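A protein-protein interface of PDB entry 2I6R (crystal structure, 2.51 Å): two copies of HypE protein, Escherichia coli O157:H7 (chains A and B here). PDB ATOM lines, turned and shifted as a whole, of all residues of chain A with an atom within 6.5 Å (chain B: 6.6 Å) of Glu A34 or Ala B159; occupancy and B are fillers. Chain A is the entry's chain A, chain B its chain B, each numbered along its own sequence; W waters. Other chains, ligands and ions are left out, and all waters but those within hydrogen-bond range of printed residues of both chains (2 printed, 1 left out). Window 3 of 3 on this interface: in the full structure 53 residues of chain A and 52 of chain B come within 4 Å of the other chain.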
ATOM      1  N   LEU A  30     -11.296  22.537   8.137  1.00  0.00           N
ATOM      2  CA  LEU A  30     -10.977  21.309   8.866  1.00  0.00           C
ATOM      3  C   LEU A  30     -12.209  20.612   9.444  1.00  0.00           C
ATOM      4  O   LEU A  30     -12.225  19.393   9.546  1.00  0.00           O
ATOM      5  CB  LEU A  30      -9.991  21.596  10.002  1.00  0.00           C
ATOM      6  CG  LEU A  30      -8.518  21.200   9.930  1.00  0.00           C
ATOM      7  CD1 LEU A  30      -8.011  21.115  11.351  1.00  0.00           C
ATOM      8  CD2 LEU A  30      -8.259  19.882   9.212  1.00  0.00           C
ATOM      9  N   ALA A  31     -13.224  21.396   9.817  1.00  0.00           N
ATOM     10  CA  ALA A  31     -14.477  20.916  10.456  1.00  0.00           C
ATOM     11  C   ALA A  31     -15.001  19.550   9.976  1.00  0.00           C
ATOM     12  O   ALA A  31     -16.047  19.454   9.310  1.00  0.00           O
ATOM     13  CB  ALA A  31     -15.586  21.994  10.344  1.00  0.00           C
ATOM     14  N   GLN A  33     -14.497  17.938   7.561  1.00  0.00           N
ATOM     15  CA  GLN A  33     -13.987  17.412   6.292  1.00  0.00           C
ATOM     16  C   GLN A  33     -13.765  15.902   6.327  1.00  0.00           C
ATOM     17  O   GLN A  33     -13.578  15.313   7.403  1.00  0.00           O
ATOM     18  CB  GLN A  33     -12.679  18.117   5.877  1.00  0.00           C
ATOM     19  CG  GLN A  33     -11.376  17.411   6.332  1.00  0.00           C
ATOM     20  CD  GLN A  33     -10.106  18.052   5.760  1.00  0.00           C
ATOM     21  OE1 GLN A  33     -10.032  19.267   5.613  1.00  0.00           O
ATOM     22  NE2 GLN A  33      -9.104  17.230   5.451  1.00  0.00           N
ATOM     23  N   GLU A  34     -13.782  15.291   5.141  1.00  0.00           N
ATOM     24  CA  GLU A  34     -13.410  13.886   4.978  1.00  0.00           C
ATOM     25  C   GLU A  34     -11.918  13.753   4.625  1.00  0.00           C
ATOM     26  O   GLU A  34     -11.062  14.171   5.403  1.00  0.00           O
ATOM     27  CB  GLU A  34     -14.272  13.231   3.916  1.00  0.00           C
ATOM     28  CG  GLU A  34     -15.768  13.241   4.203  1.00  0.00           C
ATOM     29  CD  GLU A  34     -16.596  13.233   2.914  1.00  0.00           C
ATOM     30  OE1 GLU A  34     -16.014  13.455   1.822  1.00  0.00           O
ATOM     31  OE2 GLU A  34     -17.822  13.008   3.000  1.00  0.00           O
ATOM     32  N   ASP A  35     -11.612  13.196   3.453  1.00  0.00           N
ATOM     33  CA  ASP A  35     -10.227  12.874   3.088  1.00  0.00           C
ATOM     34  C   ASP A  35      -9.392  14.035   2.521  1.00  0.00           C
ATOM     35  O   ASP A  35      -8.186  13.890   2.291  1.00  0.00           O
ATOM     36  CB  ASP A  35     -10.187  11.681   2.129  1.00  0.00           C
ATOM     37  CG  ASP A  35     -10.605  10.375   2.794  1.00  0.00           C
ATOM     38  OD1 ASP A  35     -10.375  10.202   4.013  1.00  0.00           O
ATOM     39  OD2 ASP A  35     -11.157   9.513   2.089  1.00  0.00           O
ATOM     40  N   GLN A  36     -10.030  15.182   2.305  1.00  0.00           N
ATOM     41  CA  GLN A  36      -9.354  16.323   1.724  1.00  0.00           C
ATOM     42  C   GLN A  36     -10.024  17.649   2.113  1.00  0.00           C
ATOM     43  O   GLN A  36     -11.197  17.686   2.474  1.00  0.00           O
ATOM     44  CB  GLN A  36      -9.261  16.163   0.196  1.00  0.00           C
ATOM     45  CG  GLN A  36     -10.578  16.349  -0.600  1.00  0.00           C
ATOM     46  CD  GLN A  36     -11.623  15.277  -0.341  1.00  0.00           C
ATOM     47  OE1 GLN A  36     -12.743  15.584   0.051  1.00  0.00           O
ATOM     48  NE2 GLN A  36     -11.268  14.021  -0.570  1.00  0.00           N
ATOM     49  N   ALA A  37      -9.256  18.730   2.066  1.00  0.00           N
ATOM     50  CA  ALA A  37      -9.826  20.058   2.196  1.00  0.00           C
ATOM     51  C   ALA A  37     -10.400  20.491   0.843  1.00  0.00           C
ATOM     52  O   ALA A  37      -9.982  19.994  -0.217  1.00  0.00           O
ATOM     53  CB  ALA A  37      -8.795  21.026   2.677  1.00  0.00           C
ATOM     54  N   ARG A  38     -11.375  21.397   0.895  1.00  0.00           N
ATOM     55  CA  ARG A  38     -12.065  21.858  -0.301  1.00  0.00           C
ATOM     56  C   ARG A  38     -12.053  23.384  -0.368  1.00  0.00           C
ATOM     57  O   ARG A  38     -12.698  24.053   0.443  1.00  0.00           O
ATOM     58  CB  ARG A  38     -13.484  21.281  -0.347  1.00  0.00           C
ATOM     59  CG  ARG A  38     -13.471  19.789  -0.572  1.00  0.00           C
ATOM     60  CD  ARG A  38     -14.852  19.180  -0.581  1.00  0.00           C
ATOM     61  NE  ARG A  38     -14.748  17.727  -0.476  1.00  0.00           N
ATOM     62  CZ  ARG A  38     -15.664  16.866  -0.905  1.00  0.00           C
ATOM     63  NH1 ARG A  38     -16.774  17.313  -1.477  1.00  0.00           N
ATOM     64  NH2 ARG A  38     -15.464  15.559  -0.761  1.00  0.00           N
ATOM     65  N   THR A 127      -5.831  21.032   6.322  1.00  0.00           N
ATOM     66  CA  THR A 127      -5.775  19.569   6.276  1.00  0.00           C
ATOM     67  C   THR A 127      -4.470  19.070   6.874  1.00  0.00           C
ATOM     68  O   THR A 127      -3.491  19.805   6.948  1.00  0.00           O
ATOM     69  CB  THR A 127      -5.995  19.008   4.834  1.00  0.00           C
ATOM     70  OG1 THR A 127      -6.346  17.621   4.911  1.00  0.00           O
ATOM     71  CG2 THR A 127      -4.765  19.153   3.968  1.00  0.00           C
ATOM     72  N   VAL B  84     -10.939  10.814  -4.466  1.00  0.00           N
ATOM     73  CA  VAL B  84     -12.138  10.438  -3.759  1.00  0.00           C
ATOM     74  C   VAL B  84     -13.175  11.573  -3.672  1.00  0.00           C
ATOM     75  O   VAL B  84     -14.352  11.332  -3.424  1.00  0.00           O
ATOM     76  CB  VAL B  84     -11.707   9.833  -2.405  1.00  0.00           C
ATOM     77  CG1 VAL B  84     -12.349  10.493  -1.242  1.00  0.00           C
ATOM     78  CG2 VAL B  84     -11.867   8.318  -2.414  1.00  0.00           C
ATOM     79  N   SER B  85     -12.743  12.807  -3.906  1.00  0.00           N
ATOM     80  CA  SER B  85     -13.659  13.949  -3.978  1.00  0.00           C
ATOM     81  C   SER B  85     -14.332  14.086  -5.348  1.00  0.00           C
ATOM     82  O   SER B  85     -15.315  14.825  -5.487  1.00  0.00           O
ATOM     83  CB  SER B  85     -12.922  15.256  -3.645  1.00  0.00           C
ATOM     84  OG  SER B  85     -12.113  15.699  -4.728  1.00  0.00           O
ATOM     85  N   TRP B 157     -20.151  14.893  -3.889  1.00  0.00           N
ATOM     86  CA  TRP B 157     -19.964  13.762  -3.003  1.00  0.00           C
ATOM     87  C   TRP B 157     -19.593  14.249  -1.611  1.00  0.00           C
ATOM     88  O   TRP B 157     -18.635  15.009  -1.448  1.00  0.00           O
ATOM     89  CB  TRP B 157     -18.885  12.818  -3.550  1.00  0.00           C
ATOM     90  CG  TRP B 157     -19.236  12.161  -4.871  1.00  0.00           C
ATOM     91  CD1 TRP B 157     -20.488  11.991  -5.400  1.00  0.00           C
ATOM     92  CD2 TRP B 157     -18.323  11.565  -5.810  1.00  0.00           C
ATOM     93  NE1 TRP B 157     -20.407  11.354  -6.606  1.00  0.00           N
ATOM     94  CE2 TRP B 157     -19.095  11.064  -6.879  1.00  0.00           C
ATOM     95  CE3 TRP B 157     -16.927  11.399  -5.848  1.00  0.00           C
ATOM     96  CZ2 TRP B 157     -18.522  10.419  -7.981  1.00  0.00           C
ATOM     97  CZ3 TRP B 157     -16.356  10.755  -6.948  1.00  0.00           C
ATOM     98  CH2 TRP B 157     -17.155  10.273  -7.996  1.00  0.00           C
ATOM     99  N   GLY B 158     -20.355  13.812  -0.611  1.00  0.00           N
ATOM    100  CA  GLY B 158     -20.069  14.123   0.787  1.00  0.00           C
ATOM    101  C   GLY B 158     -20.917  13.285   1.714  1.00  0.00           C
ATOM    102  O   GLY B 158     -22.076  13.007   1.416  1.00  0.00           O
ATOM    103  N   ALA B 159     -20.341  12.885   2.843  1.00  0.00           N
ATOM    104  CA  ALA B 159     -21.030  12.054   3.827  1.00  0.00           C
ATOM    105  C   ALA B 159     -22.200  12.753   4.518  1.00  0.00           C
ATOM    106  O   ALA B 159     -23.096  12.078   5.031  1.00  0.00           O
ATOM    107  CB  ALA B 159     -20.051  11.545   4.854  1.00  0.00           C
ATOM    108  N   GLN B 160     -22.197  14.087   4.539  1.00  0.00           N
ATOM    109  CA  GLN B 160     -23.286  14.859   5.147  1.00  0.00           C
ATOM    110  C   GLN B 160     -24.623  14.615   4.435  1.00  0.00           C
ATOM    111  O   GLN B 160     -25.696  14.809   5.026  1.00  0.00           O
ATOM    112  CB  GLN B 160     -22.972  16.375   5.137  1.00  0.00           C
ATOM    113  CG  GLN B 160     -21.989  16.863   6.212  1.00  0.00           C
ATOM    114  CD  GLN B 160     -21.915  18.405   6.319  1.00  0.00           C
ATOM    115  OE1 GLN B 160     -20.888  19.014   5.994  1.00  0.00           O
ATOM    116  NE2 GLN B 160     -23.009  19.032   6.779  1.00  0.00           N
ATOM    117  N   THR B 161     -24.550  14.197   3.167  1.00  0.00           N
ATOM    118  CA  THR B 161     -25.752  14.027   2.331  1.00  0.00           C
ATOM    119  C   THR B 161     -26.515  12.725   2.565  1.00  0.00           C
ATOM    120  O   THR B 161     -27.626  12.578   2.054  1.00  0.00           O
ATOM    121  CB  THR B 161     -25.453  14.149   0.807  1.00  0.00           C
ATOM    122  OG1 THR B 161     -24.538  13.122   0.400  1.00  0.00           O
ATOM    123  CG2 THR B 161     -24.878  15.531   0.458  1.00  0.00           C
ATOM    124  N   LEU B 162     -25.938  11.796   3.336  1.00  0.00           N
ATOM    125  CA  LEU B 162     -26.545  10.468   3.544  1.00  0.00           C
ATOM    126  C   LEU B 162     -27.812  10.500   4.370  1.00  0.00           C
ATOM    127  O   LEU B 162     -27.910  11.242   5.352  1.00  0.00           O
ATOM    128  CB  LEU B 162     -25.556   9.490   4.187  1.00  0.00           C
ATOM    129  CG  LEU B 162     -24.214   9.303   3.483  1.00  0.00           C
ATOM    130  CD1 LEU B 162     -23.465   8.116   4.084  1.00  0.00           C
ATOM    131  CD2 LEU B 162     -24.409   9.149   1.976  1.00  0.00           C
ATOM    132  N   THR B 163     -28.782   9.684   3.965  1.00  0.00           N
ATOM    133  CA  THR B 163     -30.060   9.572   4.659  1.00  0.00           C
ATOM    134  C   THR B 163     -30.442   8.103   4.730  1.00  0.00           C
ATOM    135  O   THR B 163     -29.922   7.285   3.964  1.00  0.00           O
ATOM    136  CB  THR B 163     -31.208  10.386   3.943  1.00  0.00           C
ATOM    137  OG1 THR B 163     -31.266  10.028   2.557  1.00  0.00           O
ATOM    138  CG2 THR B 163     -31.009  11.923   4.082  1.00  0.00           C
ATOM    139  N   LYS B 215     -23.259   9.043  -3.634  1.00  0.00           N
ATOM    140  CA  LYS B 215     -23.495  10.091  -2.641  1.00  0.00           C
ATOM    141  C   LYS B 215     -22.300  10.444  -1.789  1.00  0.00           C
ATOM    142  O   LYS B 215     -22.150  11.591  -1.394  1.00  0.00           O
ATOM    143  CB  LYS B 215     -24.702   9.740  -1.767  1.00  0.00           C
ATOM    144  CG  LYS B 215     -26.031   9.856  -2.529  1.00  0.00           C
ATOM    145  CD  LYS B 215     -27.220   9.642  -1.617  1.00  0.00           C
ATOM    146  CE  LYS B 215     -27.558  10.896  -0.803  1.00  0.00           C
ATOM    147  NZ  LYS B 215     -28.577  10.586   0.233  1.00  0.00           N
ATOM    148  N   ALA B 216     -21.451   9.461  -1.504  1.00  0.00           N
ATOM    149  CA  ALA B 216     -20.261   9.694  -0.704  1.00  0.00           C
ATOM    150  C   ALA B 216     -19.211   8.647  -1.008  1.00  0.00           C
ATOM    151  O   ALA B 216     -19.526   7.491  -1.290  1.00  0.00           O
ATOM    152  CB  ALA B 216     -20.596   9.712   0.781  1.00  0.00           C
ATOM    153  N   LEU B 217     -17.958   9.066  -0.946  1.00  0.00           N
ATOM    154  CA  LEU B 217     -16.851   8.224  -1.290  1.00  0.00           C
ATOM    155  C   LEU B 217     -15.708   8.537  -0.364  1.00  0.00           C
ATOM    156  O   LEU B 217     -15.382   9.692  -0.143  1.00  0.00           O
ATOM    157  CB  LEU B 217     -16.405   8.530  -2.704  1.00  0.00           C
ATOM    158  CG  LEU B 217     -16.160   7.345  -3.607  1.00  0.00           C
ATOM    159  CD1 LEU B 217     -17.404   7.198  -4.434  1.00  0.00           C
ATOM    160  CD2 LEU B 217     -14.987   7.640  -4.508  1.00  0.00           C
ATOM    161  N   ARG B 218     -15.080   7.499   0.154  1.00  0.00           N
ATOM    162  CA  ARG B 218     -13.945   7.654   1.038  1.00  0.00           C
ATOM    163  C   ARG B 218     -12.986   6.552   0.708  1.00  0.00           C
ATOM    164  O   ARG B 218     -13.412   5.487   0.272  1.00  0.00           O
ATOM    165  CB  ARG B 218     -14.397   7.460   2.477  1.00  0.00           C
ATOM    166  CG  ARG B 218     -14.939   8.690   3.125  1.00  0.00           C
ATOM    167  CD  ARG B 218     -13.839   9.370   3.873  1.00  0.00           C
ATOM    168  NE  ARG B 218     -14.341  10.006   5.075  1.00  0.00           N
ATOM    169  CZ  ARG B 218     -13.571  10.344   6.097  1.00  0.00           C
ATOM    170  NH1 ARG B 218     -12.261  10.100   6.057  1.00  0.00           N
ATOM    171  NH2 ARG B 218     -14.113  10.925   7.157  1.00  0.00           N
ATOM    172  N   GLU B 231     -17.305   7.615  10.718  1.00  0.00           N
ATOM    173  CA  GLU B 231     -17.213   8.990  10.204  1.00  0.00           C
ATOM    174  C   GLU B 231     -18.428   9.351   9.374  1.00  0.00           C
ATOM    175  O   GLU B 231     -18.933  10.464   9.467  1.00  0.00           O
ATOM    176  CB  GLU B 231     -15.942   9.189   9.394  1.00  0.00           C
ATOM    177  CG  GLU B 231     -14.727   9.431  10.260  1.00  0.00           C
ATOM    178  CD  GLU B 231     -13.451   8.872   9.655  1.00  0.00           C
ATOM    179  OE1 GLU B 231     -13.441   8.515   8.445  1.00  0.00           O
ATOM    180  OE2 GLU B 231     -12.452   8.779  10.404  1.00  0.00           O
ATOM    181  N   PHE B 232     -18.907   8.389   8.590  1.00  0.00           N
ATOM    182  CA  PHE B 232     -20.147   8.537   7.842  1.00  0.00           C
ATOM    183  C   PHE B 232     -21.307   8.791   8.775  1.00  0.00           C
ATOM    184  O   PHE B 232     -22.074   9.721   8.565  1.00  0.00           O
ATOM    185  CB  PHE B 232     -20.422   7.288   7.006  1.00  0.00           C
ATOM    186  CG  PHE B 232     -19.764   7.297   5.655  1.00  0.00           C
ATOM    187  CD1 PHE B 232     -18.909   8.330   5.276  1.00  0.00           C
ATOM    188  CD2 PHE B 232     -19.981   6.258   4.763  1.00  0.00           C
ATOM    189  CE1 PHE B 232     -18.300   8.342   4.026  1.00  0.00           C
ATOM    190  CE2 PHE B 232     -19.369   6.262   3.500  1.00  0.00           C
ATOM    191  CZ  PHE B 232     -18.523   7.312   3.137  1.00  0.00           C
ATOM    192  N   ALA B 233     -21.421   7.979   9.822  1.00  0.00           N
ATOM    193  CA  ALA B 233     -22.550   8.094  10.755  1.00  0.00           C
ATOM    194  C   ALA B 233     -22.571   9.429  11.506  1.00  0.00           C
ATOM    195  O   ALA B 233     -23.639   9.984  11.749  1.00  0.00           O
ATOM    196  CB  ALA B 233     -22.581   6.915  11.725  1.00  0.00           C
ATOM    197  N   ALA B 235     -21.116  12.320  10.401  1.00  0.00           N
ATOM    198  CA  ALA B 235     -21.343  13.376   9.408  1.00  0.00           C
ATOM    199  C   ALA B 235     -22.822  13.599   9.061  1.00  0.00           C
ATOM    200  O   ALA B 235     -23.239  14.740   8.861  1.00  0.00           O
ATOM    201  CB  ALA B 235     -20.547  13.096   8.142  1.00  0.00           C
ATOM    202  N   CYS B 236     -23.609  12.523   9.005  1.00  0.00           N
ATOM    203  CA  CYS B 236     -24.984  12.594   8.484  1.00  0.00           C
ATOM    204  C   CYS B 236     -26.068  12.434   9.542  1.00  0.00           C
ATOM    205  O   CYS B 236     -27.241  12.646   9.259  1.00  0.00           O
ATOM    206  CB  CYS B 236     -25.195  11.536   7.397  1.00  0.00           C
ATOM    207  SG  CYS B 236     -25.267   9.837   8.037  1.00  0.00           S
ATOM    208  N   GLY B 237     -25.677  12.032  10.746  1.00  0.00           N
ATOM    209  CA  GLY B 237     -26.622  11.885  11.849  1.00  0.00           C
ATOM    210  C   GLY B 237     -27.571  10.712  11.683  1.00  0.00           C
ATOM    211  O   GLY B 237     -28.684  10.730  12.202  1.00  0.00           O
HETATM  212  O   HOH W   1     -17.372  16.249  -4.247  1.00  0.00           O
HETATM  213  O   HOH W   2     -14.235  13.276   8.507  1.00  0.00           O
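The backbone NH (N) of Ala B159 sits at hydrogen-bond distance from the side-chain carboxylate (OE2) of Glu A34 (2.5 Å). The side-chain carboxylate (OD1) of Asp A35 lies within salt-bridge range of the guanidinium group (NH1) of Arg B218, at 2.8 Å. NH1 of Arg A38 sits at hydrogen-bond distance from O of Trp B157, 3.0 Å away.
No position is printed for both chains.
OE1 of Glu A34 lies within salt-bridge range of NH2 of Arg A38 (3.4 Å). The side-chain amide oxygen (OE1) of Gln A36 lies within hydrogen-bond range of the guanidinium group (NH2) of Arg A38 (2.8 Å). The side-chain hydroxyl of Thr B161 is in hydrogen-bond range of the backbone carbonyl oxygen of Gly B158, at 2.7 Å. The backbone carbonyl oxygen (O) of Lys B215 sits at hydrogen-bond distance from the backbone NH (N) of Gly B158, 3.0 Å away. NH2 of Arg B218 lies within salt-bridge range of OE1 of Glu B231.
Glu A34 touches three residues of chain B. Ala B159 touches just one residue of chain A: Glu A34. Of the printed residues of chain A, Val B84 touches Asp A35 and Gln A36. Printed residues of chain B within 4 Å of Asp A35: Val B84 (3.7 Å) and Arg B218 (2.8 Å). Printed residues of chain B within 4 Å of Gln A36: Val B84 (3.8 Å) and Ser B85 (3.6 Å). Of the printed residues of chain A, Ser B85 touches Gln A36 and Arg A38. Of the printed residues of chain B, Arg A38 touches Ser B85 and Trp B157. Ala A37 touches none of the printed residues of chain B. The nearest printed residue of chain B that does not touch Gln A36 is Leu B217 (6.0 Å).
Glu A34 touches Gly B158. Glu A34 touches Arg B218 (CB to NE, 3.4 Å). Asp A35 touches Val B84. Gln A36 touches Val B84. Gln A36 touches Ser B85. Arg A38 touches Ser B85 (NH2 to CB, 3.9 Å).
Water W2 bridges O of Gln A33 (2.4 Å) and NH2 of Arg B218 (2.7 Å). Water W1 lies within hydrogen-bond range of O of Ser B85, NH1 of Arg A38 and N of Trp B157.
Of the 19 printed residues of chain B, 6 touch a printed residue of chain A. Hydrophobic or aromatic side chains of chain B within 4 Å of the printed part of chain A: Val B84 and Ala B159.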
